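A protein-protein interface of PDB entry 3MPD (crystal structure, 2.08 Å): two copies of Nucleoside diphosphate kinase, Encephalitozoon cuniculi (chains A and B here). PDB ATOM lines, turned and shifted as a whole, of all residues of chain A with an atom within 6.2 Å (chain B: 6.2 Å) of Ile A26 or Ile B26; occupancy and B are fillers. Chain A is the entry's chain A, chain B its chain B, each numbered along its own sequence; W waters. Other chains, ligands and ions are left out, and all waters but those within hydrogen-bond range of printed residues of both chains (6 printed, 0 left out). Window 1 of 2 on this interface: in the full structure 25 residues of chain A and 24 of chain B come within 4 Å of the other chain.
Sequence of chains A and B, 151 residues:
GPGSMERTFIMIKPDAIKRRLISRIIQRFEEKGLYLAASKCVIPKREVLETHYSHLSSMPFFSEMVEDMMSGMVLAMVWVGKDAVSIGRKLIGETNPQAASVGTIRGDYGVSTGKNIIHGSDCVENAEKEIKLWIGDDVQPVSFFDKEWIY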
ATOM      1  N   ILE A  12     -13.800  -4.911 -32.609  1.00  0.00           N
ATOM      2  CA  ILE A  12     -13.397  -6.193 -32.030  1.00  0.00           C
ATOM      3  C   ILE A  12     -13.068  -7.152 -33.172  1.00  0.00           C
ATOM      4  O   ILE A  12     -13.931  -7.403 -34.041  1.00  0.00           O
ATOM      5  CB  ILE A  12     -14.482  -6.803 -31.119  1.00  0.00           C
ATOM      6  CG1 ILE A  12     -14.885  -5.801 -30.031  1.00  0.00           C
ATOM      7  CG2 ILE A  12     -14.016  -8.198 -30.543  1.00  0.00           C
ATOM      8  CD1 ILE A  12     -15.933  -6.362 -29.023  1.00  0.00           C
ATOM      9  N   LEU A  21     -15.197 -12.555 -25.993  1.00  0.00           N
ATOM     10  CA  LEU A  21     -14.666 -11.414 -25.246  1.00  0.00           C
ATOM     11  C   LEU A  21     -15.484 -10.135 -25.394  1.00  0.00           C
ATOM     12  O   LEU A  21     -15.064  -9.063 -24.912  1.00  0.00           O
ATOM     13  CB  LEU A  21     -13.202 -11.145 -25.685  1.00  0.00           C
ATOM     14  CG  LEU A  21     -12.195 -12.199 -25.252  1.00  0.00           C
ATOM     15  CD1 LEU A  21     -10.837 -12.006 -25.961  1.00  0.00           C
ATOM     16  CD2 LEU A  21     -11.964 -12.085 -23.745  1.00  0.00           C
ATOM     17  N   ILE A  22     -16.623 -10.209 -26.066  1.00  0.00           N
ATOM     18  CA  ILE A  22     -17.423  -8.999 -26.303  1.00  0.00           C
ATOM     19  C   ILE A  22     -17.764  -8.230 -25.009  1.00  0.00           C
ATOM     20  O   ILE A  22     -17.480  -7.039 -24.918  1.00  0.00           O
ATOM     21  CB  ILE A  22     -18.721  -9.265 -27.124  1.00  0.00           C
ATOM     22  CG1 ILE A  22     -18.378  -9.855 -28.503  1.00  0.00           C
ATOM     23  CG2 ILE A  22     -19.547  -7.924 -27.320  1.00  0.00           C
ATOM     24  CD1 ILE A  22     -19.649 -10.384 -29.254  1.00  0.00           C
ATOM     25  N   SER A  23     -18.357  -8.883 -24.014  1.00  0.00           N
ATOM     26  CA  SER A  23     -18.821  -8.127 -22.824  1.00  0.00           C
ATOM     27  C   SER A  23     -17.655  -7.554 -22.030  1.00  0.00           C
ATOM     28  O   SER A  23     -17.761  -6.452 -21.499  1.00  0.00           O
ATOM     29  CB  SER A  23     -19.721  -8.940 -21.877  1.00  0.00           C
ATOM     30  OG  SER A  23     -18.988  -9.984 -21.262  1.00  0.00           O
ATOM     31  N   ARG A  24     -16.559  -8.310 -21.957  1.00  0.00           N
ATOM     32  CA  ARG A  24     -15.362  -7.883 -21.227  1.00  0.00           C
ATOM     33  C   ARG A  24     -14.696  -6.661 -21.865  1.00  0.00           C
ATOM     34  O   ARG A  24     -14.137  -5.806 -21.188  1.00  0.00           O
ATOM     35  CB  ARG A  24     -14.359  -9.056 -21.103  1.00  0.00           C
ATOM     36  CG  ARG A  24     -14.728  -9.962 -19.889  1.00  0.00           C
ATOM     37  CD  ARG A  24     -13.985 -11.304 -19.892  1.00  0.00           C
ATOM     38  NE  ARG A  24     -14.488 -12.245 -20.904  1.00  0.00           N
ATOM     39  CZ  ARG A  24     -14.030 -13.504 -21.058  1.00  0.00           C
ATOM     40  NH1 ARG A  24     -13.055 -13.974 -20.265  1.00  0.00           N
ATOM     41  NH2 ARG A  24     -14.544 -14.305 -21.996  1.00  0.00           N
ATOM     42  N   ILE A  25     -14.706  -6.620 -23.180  1.00  0.00           N
ATOM     43  CA  ILE A  25     -14.155  -5.482 -23.920  1.00  0.00           C
ATOM     44  C   ILE A  25     -15.079  -4.239 -23.758  1.00  0.00           C
ATOM     45  O   ILE A  25     -14.624  -3.152 -23.453  1.00  0.00           O
ATOM     46  CB  ILE A  25     -14.000  -5.869 -25.401  1.00  0.00           C
ATOM     47  CG1 ILE A  25     -12.777  -6.806 -25.583  1.00  0.00           C
ATOM     48  CG2 ILE A  25     -13.906  -4.618 -26.291  1.00  0.00           C
ATOM     49  CD1 ILE A  25     -12.828  -7.604 -26.917  1.00  0.00           C
ATOM     50  N   ILE A  26     -16.366  -4.403 -23.958  1.00  0.00           N
ATOM     51  CA  ILE A  26     -17.278  -3.268 -23.851  1.00  0.00           C
ATOM     52  C   ILE A  26     -17.267  -2.686 -22.429  1.00  0.00           C
ATOM     53  O   ILE A  26     -17.369  -1.465 -22.249  1.00  0.00           O
ATOM     54  CB  ILE A  26     -18.698  -3.681 -24.300  1.00  0.00           C
ATOM     55  CG1 ILE A  26     -18.688  -3.928 -25.841  1.00  0.00           C
ATOM     56  CG2 ILE A  26     -19.741  -2.591 -23.889  1.00  0.00           C
ATOM     57  CD1 ILE A  26     -20.066  -4.367 -26.395  1.00  0.00           C
ATOM     58  N   GLN A  27     -17.165  -3.550 -21.421  1.00  0.00           N
ATOM     59  CA  GLN A  27     -17.059  -3.078 -20.031  1.00  0.00           C
ATOM     60  C   GLN A  27     -15.953  -2.030 -19.853  1.00  0.00           C
ATOM     61  O   GLN A  27     -16.160  -1.050 -19.118  1.00  0.00           O
ATOM     62  CB  GLN A  27     -16.803  -4.251 -19.059  1.00  0.00           C
ATOM     63  CG  GLN A  27     -16.757  -3.870 -17.568  1.00  0.00           C
ATOM     64  CD  GLN A  27     -16.363  -5.093 -16.642  1.00  0.00           C
ATOM     65  OE1 GLN A  27     -16.553  -6.248 -16.991  1.00  0.00           O
ATOM     66  NE2 GLN A  27     -15.809  -4.805 -15.502  1.00  0.00           N
ATOM     67  N   ARG A  28     -14.789  -2.236 -20.485  1.00  0.00           N
ATOM     68  CA  ARG A  28     -13.656  -1.303 -20.283  1.00  0.00           C
ATOM     69  C   ARG A  28     -14.042   0.107 -20.750  1.00  0.00           C
ATOM     70  O   ARG A  28     -13.718   1.091 -20.089  1.00  0.00           O
ATOM     71  CB  ARG A  28     -12.372  -1.728 -21.001  1.00  0.00           C
ATOM     72  CG  ARG A  28     -11.955  -3.206 -20.844  1.00  0.00           C
ATOM     73  CD  ARG A  28     -11.569  -3.483 -19.415  1.00  0.00           C
ATOM     74  NE  ARG A  28     -11.050  -4.852 -19.223  1.00  0.00           N
ATOM     75  CZ  ARG A  28      -9.770  -5.227 -19.269  1.00  0.00           C
ATOM     76  NH1 ARG A  28      -8.811  -4.364 -19.560  1.00  0.00           N
ATOM     77  NH2 ARG A  28      -9.455  -6.486 -18.983  1.00  0.00           N
ATOM     78  N   PHE A  29     -14.716   0.183 -21.894  1.00  0.00           N
ATOM     79  CA  PHE A  29     -15.100   1.466 -22.479  1.00  0.00           C
ATOM     80  C   PHE A  29     -16.254   2.130 -21.732  1.00  0.00           C
ATOM     81  O   PHE A  29     -16.277   3.365 -21.521  1.00  0.00           O
ATOM     82  CB  PHE A  29     -15.444   1.286 -23.965  1.00  0.00           C
ATOM     83  CG  PHE A  29     -14.238   1.039 -24.802  1.00  0.00           C
ATOM     84  CD1 PHE A  29     -13.638   2.091 -25.476  1.00  0.00           C
ATOM     85  CD2 PHE A  29     -13.668  -0.237 -24.889  1.00  0.00           C
ATOM     86  CE1 PHE A  29     -12.483   1.878 -26.221  1.00  0.00           C
ATOM     87  CE2 PHE A  29     -12.485  -0.444 -25.652  1.00  0.00           C
ATOM     88  CZ  PHE A  29     -11.913   0.625 -26.296  1.00  0.00           C
ATOM     89  N   GLU A  30     -17.221   1.314 -21.347  1.00  0.00           N
ATOM     90  CA  GLU A  30     -18.443   1.814 -20.730  1.00  0.00           C
ATOM     91  C   GLU A  30     -18.121   2.272 -19.292  1.00  0.00           C
ATOM     92  O   GLU A  30     -18.651   3.282 -18.828  1.00  0.00           O
ATOM     93  CB  GLU A  30     -19.503   0.680 -20.751  1.00  0.00           C
ATOM     94  CG  GLU A  30     -20.856   1.039 -20.158  1.00  0.00           C
ATOM     95  CD  GLU A  30     -21.920  -0.060 -20.321  1.00  0.00           C
ATOM     96  OE1 GLU A  30     -21.631  -1.282 -20.127  1.00  0.00           O
ATOM     97  OE2 GLU A  30     -23.088   0.319 -20.568  1.00  0.00           O
ATOM     98  N   GLU A  31     -17.231   1.543 -18.593  1.00  0.00           N
ATOM     99  CA  GLU A  31     -16.857   1.920 -17.201  1.00  0.00           C
ATOM    100  C   GLU A  31     -15.945   3.129 -17.160  1.00  0.00           C
ATOM    101  O   GLU A  31     -15.912   3.848 -16.145  1.00  0.00           O
ATOM    102  CB  GLU A  31     -16.207   0.752 -16.419  1.00  0.00           C
ATOM    103  CG  GLU A  31     -17.202  -0.293 -16.016  1.00  0.00           C
ATOM    104  CD  GLU A  31     -16.593  -1.436 -15.188  1.00  0.00           C
ATOM    105  OE1 GLU A  31     -15.358  -1.752 -15.269  1.00  0.00           O
ATOM    106  OE2 GLU A  31     -17.399  -2.064 -14.488  1.00  0.00           O
ATOM    107  N   LEU A  36     -21.274   4.918 -26.143  1.00  0.00           N
ATOM    108  CA  LEU A  36     -21.495   4.161 -27.375  1.00  0.00           C
ATOM    109  C   LEU A  36     -22.452   4.908 -28.305  1.00  0.00           C
ATOM    110  O   LEU A  36     -23.543   5.309 -27.869  1.00  0.00           O
ATOM    111  CB  LEU A  36     -22.045   2.766 -27.042  1.00  0.00           C
ATOM    112  CG  LEU A  36     -22.278   1.835 -28.231  1.00  0.00           C
ATOM    113  CD1 LEU A  36     -20.927   1.515 -28.897  1.00  0.00           C
ATOM    114  CD2 LEU A  36     -23.002   0.560 -27.812  1.00  0.00           C
ATOM    115  N   LEU A  75     -17.120  -6.871 -34.629  1.00  0.00           N
ATOM    116  CA  LEU A  75     -18.055  -5.878 -34.075  1.00  0.00           C
ATOM    117  C   LEU A  75     -17.464  -4.470 -34.151  1.00  0.00           C
ATOM    118  O   LEU A  75     -16.531  -4.126 -33.400  1.00  0.00           O
ATOM    119  CB  LEU A  75     -18.487  -6.231 -32.636  1.00  0.00           C
ATOM    120  CG  LEU A  75     -19.523  -5.312 -31.950  1.00  0.00           C
ATOM    121  CD1 LEU A  75     -20.857  -5.317 -32.717  1.00  0.00           C
ATOM    122  CD2 LEU A  75     -19.747  -5.727 -30.491  1.00  0.00           C
ATOM    123  N   MET A  77     -17.678  -0.410 -33.798  1.00  0.00           N
ATOM    124  CA  MET A  77     -18.344   0.549 -32.901  1.00  0.00           C
ATOM    125  C   MET A  77     -17.772   1.939 -33.012  1.00  0.00           C
ATOM    126  O   MET A  77     -16.597   2.116 -33.346  1.00  0.00           O
ATOM    127  CB  MET A  77     -18.157   0.116 -31.410  1.00  0.00           C
ATOM    128  CG  MET A  77     -18.897  -1.151 -31.048  1.00  0.00           C
ATOM    129  SD  MET A  77     -18.395  -1.940 -29.486  1.00  0.00           S
ATOM    130  CE  MET A  77     -16.845  -2.685 -29.925  1.00  0.00           C
ATOM    131  N   TRP A  79     -17.344   5.124 -30.293  1.00  0.00           N
ATOM    132  CA  TRP A  79     -17.427   5.553 -28.907  1.00  0.00           C
ATOM    133  C   TRP A  79     -17.069   7.034 -28.855  1.00  0.00           C
ATOM    134  O   TRP A  79     -16.104   7.461 -29.488  1.00  0.00           O
ATOM    135  CB  TRP A  79     -16.472   4.725 -28.027  1.00  0.00           C
ATOM    136  CG  TRP A  79     -16.938   3.327 -27.775  1.00  0.00           C
ATOM    137  CD1 TRP A  79     -16.740   2.229 -28.586  1.00  0.00           C
ATOM    138  CD2 TRP A  79     -17.696   2.851 -26.637  1.00  0.00           C
ATOM    139  NE1 TRP A  79     -17.309   1.102 -28.003  1.00  0.00           N
ATOM    140  CE2 TRP A  79     -17.894   1.453 -26.816  1.00  0.00           C
ATOM    141  CE3 TRP A  79     -18.222   3.467 -25.496  1.00  0.00           C
ATOM    142  CZ2 TRP A  79     -18.600   0.670 -25.900  1.00  0.00           C
ATOM    143  CZ3 TRP A  79     -18.915   2.690 -24.582  1.00  0.00           C
ATOM    144  CH2 TRP A  79     -19.111   1.299 -24.796  1.00  0.00           C
ATOM    145  N   ILE B  12     -31.902  -3.442 -25.733  1.00  0.00           N
ATOM    146  CA  ILE B  12     -31.670  -2.766 -24.459  1.00  0.00           C
ATOM    147  C   ILE B  12     -32.381  -1.410 -24.493  1.00  0.00           C
ATOM    148  O   ILE B  12     -32.127  -0.583 -25.388  1.00  0.00           O
ATOM    149  CB  ILE B  12     -30.162  -2.573 -24.182  1.00  0.00           C
ATOM    150  CG1 ILE B  12     -29.462  -3.940 -24.168  1.00  0.00           C
ATOM    151  CG2 ILE B  12     -29.961  -1.834 -22.858  1.00  0.00           C
ATOM    152  CD1 ILE B  12     -27.951  -3.889 -23.912  1.00  0.00           C
ATOM    153  N   LEU B  21     -25.579  -0.409 -18.350  1.00  0.00           N
ATOM    154  CA  LEU B  21     -25.765  -1.845 -18.198  1.00  0.00           C
ATOM    155  C   LEU B  21     -25.447  -2.650 -19.466  1.00  0.00           C
ATOM    156  O   LEU B  21     -25.716  -3.845 -19.508  1.00  0.00           O
ATOM    157  CB  LEU B  21     -27.241  -2.102 -17.824  1.00  0.00           C
ATOM    158  CG  LEU B  21     -27.621  -1.643 -16.406  1.00  0.00           C
ATOM    159  CD1 LEU B  21     -29.163  -1.612 -16.193  1.00  0.00           C
ATOM    160  CD2 LEU B  21     -26.965  -2.551 -15.382  1.00  0.00           C
ATOM    161  N   ILE B  22     -24.871  -2.021 -20.485  1.00  0.00           N
ATOM    162  CA  ILE B  22     -24.624  -2.748 -21.743  1.00  0.00           C
ATOM    163  C   ILE B  22     -23.759  -4.026 -21.517  1.00  0.00           C
ATOM    164  O   ILE B  22     -24.156  -5.124 -21.905  1.00  0.00           O
ATOM    165  CB  ILE B  22     -23.979  -1.850 -22.848  1.00  0.00           C
ATOM    166  CG1 ILE B  22     -24.912  -0.687 -23.218  1.00  0.00           C
ATOM    167  CG2 ILE B  22     -23.613  -2.710 -24.075  1.00  0.00           C
ATOM    168  CD1 ILE B  22     -24.267   0.332 -24.195  1.00  0.00           C
ATOM    169  N   SER B  23     -22.603  -3.890 -20.885  1.00  0.00           N
ATOM    170  CA  SER B  23     -21.681  -5.049 -20.791  1.00  0.00           C
ATOM    171  C   SER B  23     -22.281  -6.177 -19.913  1.00  0.00           C
ATOM    172  O   SER B  23     -22.172  -7.356 -20.235  1.00  0.00           O
ATOM    173  CB  SER B  23     -20.309  -4.635 -20.268  1.00  0.00           C
ATOM    174  OG  SER B  23     -20.370  -4.264 -18.875  1.00  0.00           O
ATOM    175  N   ARG B  24     -22.974  -5.792 -18.848  1.00  0.00           N
ATOM    176  CA  ARG B  24     -23.593  -6.753 -17.936  1.00  0.00           C
ATOM    177  C   ARG B  24     -24.717  -7.514 -18.606  1.00  0.00           C
ATOM    178  O   ARG B  24     -24.893  -8.706 -18.379  1.00  0.00           O
ATOM    179  CB  ARG B  24     -24.057  -6.047 -16.647  1.00  0.00           C
ATOM    180  CG  ARG B  24     -22.901  -5.862 -15.644  1.00  0.00           C
ATOM    181  CD  ARG B  24     -23.284  -4.894 -14.509  1.00  0.00           C
ATOM    182  NE  ARG B  24     -23.353  -3.504 -14.967  1.00  0.00           N
ATOM    183  CZ  ARG B  24     -23.618  -2.452 -14.173  1.00  0.00           C
ATOM    184  NH1 ARG B  24     -23.830  -2.636 -12.870  1.00  0.00           N
ATOM    185  NH2 ARG B  24     -23.653  -1.207 -14.668  1.00  0.00           N
ATOM    186  N   ILE B  25     -25.448  -6.836 -19.478  1.00  0.00           N
ATOM    187  CA  ILE B  25     -26.513  -7.478 -20.242  1.00  0.00           C
ATOM    188  C   ILE B  25     -25.912  -8.425 -21.300  1.00  0.00           C
ATOM    189  O   ILE B  25     -26.340  -9.575 -21.438  1.00  0.00           O
ATOM    190  CB  ILE B  25     -27.469  -6.416 -20.900  1.00  0.00           C
ATOM    191  CG1 ILE B  25     -28.414  -5.806 -19.866  1.00  0.00           C
ATOM    192  CG2 ILE B  25     -28.254  -7.039 -22.084  1.00  0.00           C
ATOM    193  CD1 ILE B  25     -28.937  -4.424 -20.256  1.00  0.00           C
ATOM    194  N   ILE B  26     -24.945  -7.944 -22.073  1.00  0.00           N
ATOM    195  CA  ILE B  26     -24.391  -8.782 -23.138  1.00  0.00           C
ATOM    196  C   ILE B  26     -23.761 -10.043 -22.541  1.00  0.00           C
ATOM    197  O   ILE B  26     -23.852 -11.144 -23.116  1.00  0.00           O
ATOM    198  CB  ILE B  26     -23.381  -7.973 -24.026  1.00  0.00           C
ATOM    199  CG1 ILE B  26     -24.179  -7.026 -24.928  1.00  0.00           C
ATOM    200  CG2 ILE B  26     -22.510  -8.901 -24.895  1.00  0.00           C
ATOM    201  CD1 ILE B  26     -23.344  -6.092 -25.770  1.00  0.00           C
ATOM    202  N   GLN B  27     -23.128  -9.879 -21.389  1.00  0.00           N
ATOM    203  CA  GLN B  27     -22.536 -11.006 -20.677  1.00  0.00           C
ATOM    204  C   GLN B  27     -23.483 -12.197 -20.517  1.00  0.00           C
ATOM    205  O   GLN B  27     -23.054 -13.337 -20.745  1.00  0.00           O
ATOM    206  CB  GLN B  27     -21.963 -10.581 -19.314  1.00  0.00           C
ATOM    207  CG  GLN B  27     -21.299 -11.716 -18.527  1.00  0.00           C
ATOM    208  CD  GLN B  27     -20.812 -11.294 -17.126  1.00  0.00           C
ATOM    209  OE1 GLN B  27     -20.721 -10.123 -16.822  1.00  0.00           O
ATOM    210  NE2 GLN B  27     -20.481 -12.262 -16.296  1.00  0.00           N
ATOM    211  N   ARG B  28     -24.735 -11.956 -20.107  1.00  0.00           N
ATOM    212  CA  ARG B  28     -25.700 -13.035 -19.906  1.00  0.00           C
ATOM    213  C   ARG B  28     -25.907 -13.886 -21.159  1.00  0.00           C
ATOM    214  O   ARG B  28     -25.949 -15.131 -21.104  1.00  0.00           O
ATOM    215  CB  ARG B  28     -27.070 -12.482 -19.442  1.00  0.00           C
ATOM    216  CG  ARG B  28     -27.009 -11.413 -18.277  1.00  0.00           C
ATOM    217  CD  ARG B  28     -26.484 -12.035 -17.040  1.00  0.00           C
ATOM    218  NE  ARG B  28     -26.475 -11.131 -15.863  1.00  0.00           N
ATOM    219  CZ  ARG B  28     -27.419 -11.070 -14.926  1.00  0.00           C
ATOM    220  NH1 ARG B  28     -28.524 -11.803 -15.033  1.00  0.00           N
ATOM    221  NH2 ARG B  28     -27.256 -10.275 -13.863  1.00  0.00           N
ATOM    222  N   PHE B  29     -26.060 -13.218 -22.282  1.00  0.00           N
ATOM    223  CA  PHE B  29     -26.299 -13.904 -23.556  1.00  0.00           C
ATOM    224  C   PHE B  29     -25.039 -14.590 -24.040  1.00  0.00           C
ATOM    225  O   PHE B  29     -25.076 -15.724 -24.544  1.00  0.00           O
ATOM    226  CB  PHE B  29     -26.847 -12.906 -24.597  1.00  0.00           C
ATOM    227  CG  PHE B  29     -28.287 -12.497 -24.313  1.00  0.00           C
ATOM    228  CD1 PHE B  29     -29.338 -13.192 -24.886  1.00  0.00           C
ATOM    229  CD2 PHE B  29     -28.577 -11.462 -23.424  1.00  0.00           C
ATOM    230  CE1 PHE B  29     -30.670 -12.856 -24.592  1.00  0.00           C
ATOM    231  CE2 PHE B  29     -29.906 -11.112 -23.131  1.00  0.00           C
ATOM    232  CZ  PHE B  29     -30.952 -11.825 -23.716  1.00  0.00           C
ATOM    233  N   GLU B  30     -23.910 -13.907 -23.888  1.00  0.00           N
ATOM    234  CA  GLU B  30     -22.658 -14.415 -24.448  1.00  0.00           C
ATOM    235  C   GLU B  30     -22.175 -15.658 -23.647  1.00  0.00           C
ATOM    236  O   GLU B  30     -21.725 -16.661 -24.241  1.00  0.00           O
ATOM    237  CB  GLU B  30     -21.610 -13.297 -24.489  1.00  0.00           C
ATOM    238  CG  GLU B  30     -20.301 -13.696 -25.163  1.00  0.00           C
ATOM    239  CD  GLU B  30     -19.342 -12.531 -25.315  1.00  0.00           C
ATOM    240  OE1 GLU B  30     -19.245 -11.704 -24.360  1.00  0.00           O
ATOM    241  OE2 GLU B  30     -18.659 -12.472 -26.378  1.00  0.00           O
ATOM    242  N   GLU B  31     -22.330 -15.626 -22.327  1.00  0.00           N
ATOM    243  CA  GLU B  31     -21.879 -16.740 -21.468  1.00  0.00           C
ATOM    244  C   GLU B  31     -22.830 -17.936 -21.538  1.00  0.00           C
ATOM    245  O   GLU B  31     -22.430 -19.066 -21.219  1.00  0.00           O
ATOM    246  CB  GLU B  31     -21.752 -16.273 -19.993  1.00  0.00           C
ATOM    247  CG  GLU B  31     -20.541 -15.411 -19.783  1.00  0.00           C
ATOM    248  CD  GLU B  31     -20.312 -15.023 -18.300  1.00  0.00           C
ATOM    249  OE1 GLU B  31     -21.261 -15.112 -17.467  1.00  0.00           O
ATOM    250  OE2 GLU B  31     -19.157 -14.620 -17.980  1.00  0.00           O
ATOM    251  N   LEU B  36     -24.100 -13.596 -31.183  1.00  0.00           N
ATOM    252  CA  LEU B  36     -24.475 -12.289 -31.717  1.00  0.00           C
ATOM    253  C   LEU B  36     -24.373 -12.286 -33.237  1.00  0.00           C
ATOM    254  O   LEU B  36     -23.334 -12.684 -33.792  1.00  0.00           O
ATOM    255  CB  LEU B  36     -23.576 -11.206 -31.102  1.00  0.00           C
ATOM    256  CG  LEU B  36     -23.881  -9.776 -31.512  1.00  0.00           C
ATOM    257  CD1 LEU B  36     -25.216  -9.295 -30.978  1.00  0.00           C
ATOM    258  CD2 LEU B  36     -22.733  -8.913 -31.067  1.00  0.00           C
ATOM    259  N   LEU B  75     -30.017  -0.213 -27.901  1.00  0.00           N
ATOM    260  CA  LEU B  75     -29.107  -1.148 -28.592  1.00  0.00           C
ATOM    261  C   LEU B  75     -29.892  -2.385 -29.031  1.00  0.00           C
ATOM    262  O   LEU B  75     -30.316  -3.209 -28.199  1.00  0.00           O
ATOM    263  CB  LEU B  75     -27.914  -1.551 -27.702  1.00  0.00           C
ATOM    264  CG  LEU B  75     -26.877  -2.487 -28.350  1.00  0.00           C
ATOM    265  CD1 LEU B  75     -26.282  -1.834 -29.584  1.00  0.00           C
ATOM    266  CD2 LEU B  75     -25.721  -2.854 -27.318  1.00  0.00           C
ATOM    267  N   MET B  77     -30.319  -5.872 -31.139  1.00  0.00           N
ATOM    268  CA  MET B  77     -29.442  -7.012 -31.413  1.00  0.00           C
ATOM    269  C   MET B  77     -30.226  -8.219 -31.876  1.00  0.00           C
ATOM    270  O   MET B  77     -31.402  -8.373 -31.539  1.00  0.00           O
ATOM    271  CB  MET B  77     -28.689  -7.398 -30.129  1.00  0.00           C
ATOM    272  CG  MET B  77     -27.596  -6.429 -29.722  1.00  0.00           C
ATOM    273  SD  MET B  77     -26.971  -6.754 -28.034  1.00  0.00           S
ATOM    274  CE  MET B  77     -28.390  -6.319 -27.050  1.00  0.00           C
ATOM    275  N   TRP B  79     -29.711 -12.330 -31.510  1.00  0.00           N
ATOM    276  CA  TRP B  79     -28.917 -13.456 -31.013  1.00  0.00           C
ATOM    277  C   TRP B  79     -29.491 -14.749 -31.598  1.00  0.00           C
ATOM    278  O   TRP B  79     -30.711 -14.850 -31.761  1.00  0.00           O
ATOM    279  CB  TRP B  79     -28.960 -13.487 -29.488  1.00  0.00           C
ATOM    280  CG  TRP B  79     -28.206 -12.335 -28.884  1.00  0.00           C
ATOM    281  CD1 TRP B  79     -28.666 -11.045 -28.707  1.00  0.00           C
ATOM    282  CD2 TRP B  79     -26.861 -12.352 -28.409  1.00  0.00           C
ATOM    283  NE1 TRP B  79     -27.689 -10.275 -28.110  1.00  0.00           N
ATOM    284  CE2 TRP B  79     -26.569 -11.048 -27.927  1.00  0.00           C
ATOM    285  CE3 TRP B  79     -25.871 -13.344 -28.321  1.00  0.00           C
ATOM    286  CZ2 TRP B  79     -25.326 -10.710 -27.380  1.00  0.00           C
ATOM    287  CZ3 TRP B  79     -24.643 -13.010 -27.750  1.00  0.00           C
ATOM    288  CH2 TRP B  79     -24.380 -11.698 -27.308  1.00  0.00           C
HETATM  289  O   HOH W   1     -22.604  -3.027 -17.728  1.00  0.00           O
HETATM  290  O   HOH W   2     -19.475  -6.499 -17.579  1.00  0.00           O
HETATM  291  O   HOH W   3     -18.437  -9.097 -18.753  1.00  0.00           O
HETATM  292  O   HOH W   4     -19.739  -1.410 -17.872  1.00  0.00           O
HETATM  293  O   HOH W   5     -19.439 -12.969 -21.902  1.00  0.00           O
HETATM  294  O   HOH W   6     -16.730 -11.297 -22.451  1.00  0.00           O
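The backbone NH of Ser A23 sits at hydrogen-bond distance from the side-chain carboxylate of Glu B30 (3.0 Å). N of Ile B22 is in hydrogen-bond range of OE2 of Glu A30 (2.9 Å). The backbone NH of Ile A22 sits at hydrogen-bond distance from the side-chain carboxylate of Glu B30 (3.1 Å). N of Ser B23 lies within hydrogen-bond range of OE1 of Glu A30 (2.9 Å). N of Leu B21 is in hydrogen-bond range of OE2 of Glu A30 (3.4 Å). The side-chain carboxylate (OE2) of Glu B30 is in hydrogen-bond range of the backbone NH (N) of Leu A21 (3.5 Å).
CG2 of Ile A22 touches CG2 of Ile B26, at 3.95 Å. CD2 of Leu B36 touches CD1 of Ile A22, 3.9 Å away. CB of Ser A23 touches O of Ser B23, 3.3 Å away. Ser A23 touches Gln B27 (CB to N, 3.6 Å). CG2 of Ile B22 touches CG2 of Ile A26, 3.9 Å away. Ile A26 touches Ile B26. CB of Ser B23 touches N of Gln A27 (3.5 Å). Leu A36 touches Ile B22 (CD2 to CD1, 3.8 Å).
Of chain B, only Ile B22 and Ile B26 come within 4 Å of Ile A26. Of the printed residues of chain A, Ser B23 touches Ser A23 (3.3 Å), Gln A27 (3.5 Å) and Glu A30 (2.9 Å). Of the printed residues of chain A, Ile B26 touches Ile A22 and Ile A26. Printed residues of chain A within 4 Å of Leu B36: Ile A22.
Of the 16 printed residues of chain A, 7 touch a printed residue of chain B. Hydrophobic or aromatic side chains of chain A within 4 Å of the printed part of chain B: Ile A22, Ile A26 and Leu A36. Along chain A the printed residues that touch a printed residue of chain B span positions 21 to 36. Printed residues of chain B that touch a printed residue of chain A: Leu B21, Ile B22, Ser B23, Ile B26, Gln B27, Glu B30 and Leu B36. Hydrophobic or aromatic side chains of chain B within 4 Å of the printed part of chain A: Ile B22, Ile B26 and Leu B36. Among the printed residues, 14 pairs touch across the chains.
Ile A22 touches Glu B30, and with the chains exchanged Glu A30 touches Ile B22. Ser B23 touches its own counterpart, Ser A23. Ser A23 touches Glu B30, and with the chains exchanged Glu A30 touches Ser B23. Ile B26 touches its own counterpart, Ile A26. Of the 14 pairs that touch across the chains among the printed residues, 14 have their exchanged pair printed and touching as well.
Water W3 lies within hydrogen-bond range of OG of Ser A23 (2.7 Å) and OE1 of Gln B27 (3.2 Å). Water W2 bridges the side-chain hydroxyl of Ser B23 (2.7 Å) and the side-chain amide oxygen of Gln A27 (3.0 Å). Water W5 bridges the side-chain carboxylate (OE1) of Glu B30 and the side-chain hydroxyl (OG) of Ser A23. Water W1 lies within hydrogen-bond range of the side-chain hydroxyl of Ser B23 (2.8 Å), the guanidinium group of Arg B24 (2.9 Å) and the side-chain carboxylate of Glu A30 (3.1 Å). Water W6 lies within hydrogen-bond range of the side-chain hydroxyl (OG) of Ser A23, the guanidinium group (NE) of Arg A24 and the side-chain carboxylate (OE1) of Glu B30. Water W4 lies within hydrogen-bond range of OE1 of Glu A30 and OG of Ser B23.
The side-chain amide nitrogen (NE2) of Gln A27 lies within hydrogen-bond range of the side-chain carboxylate (OE1) of Glu A31, 3.1 Å away. The side-chain carboxylate (OE1) of Glu B31 is in hydrogen-bond range of the side-chain amide nitrogen (NE2) of Gln B27, at 3.2 Å.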
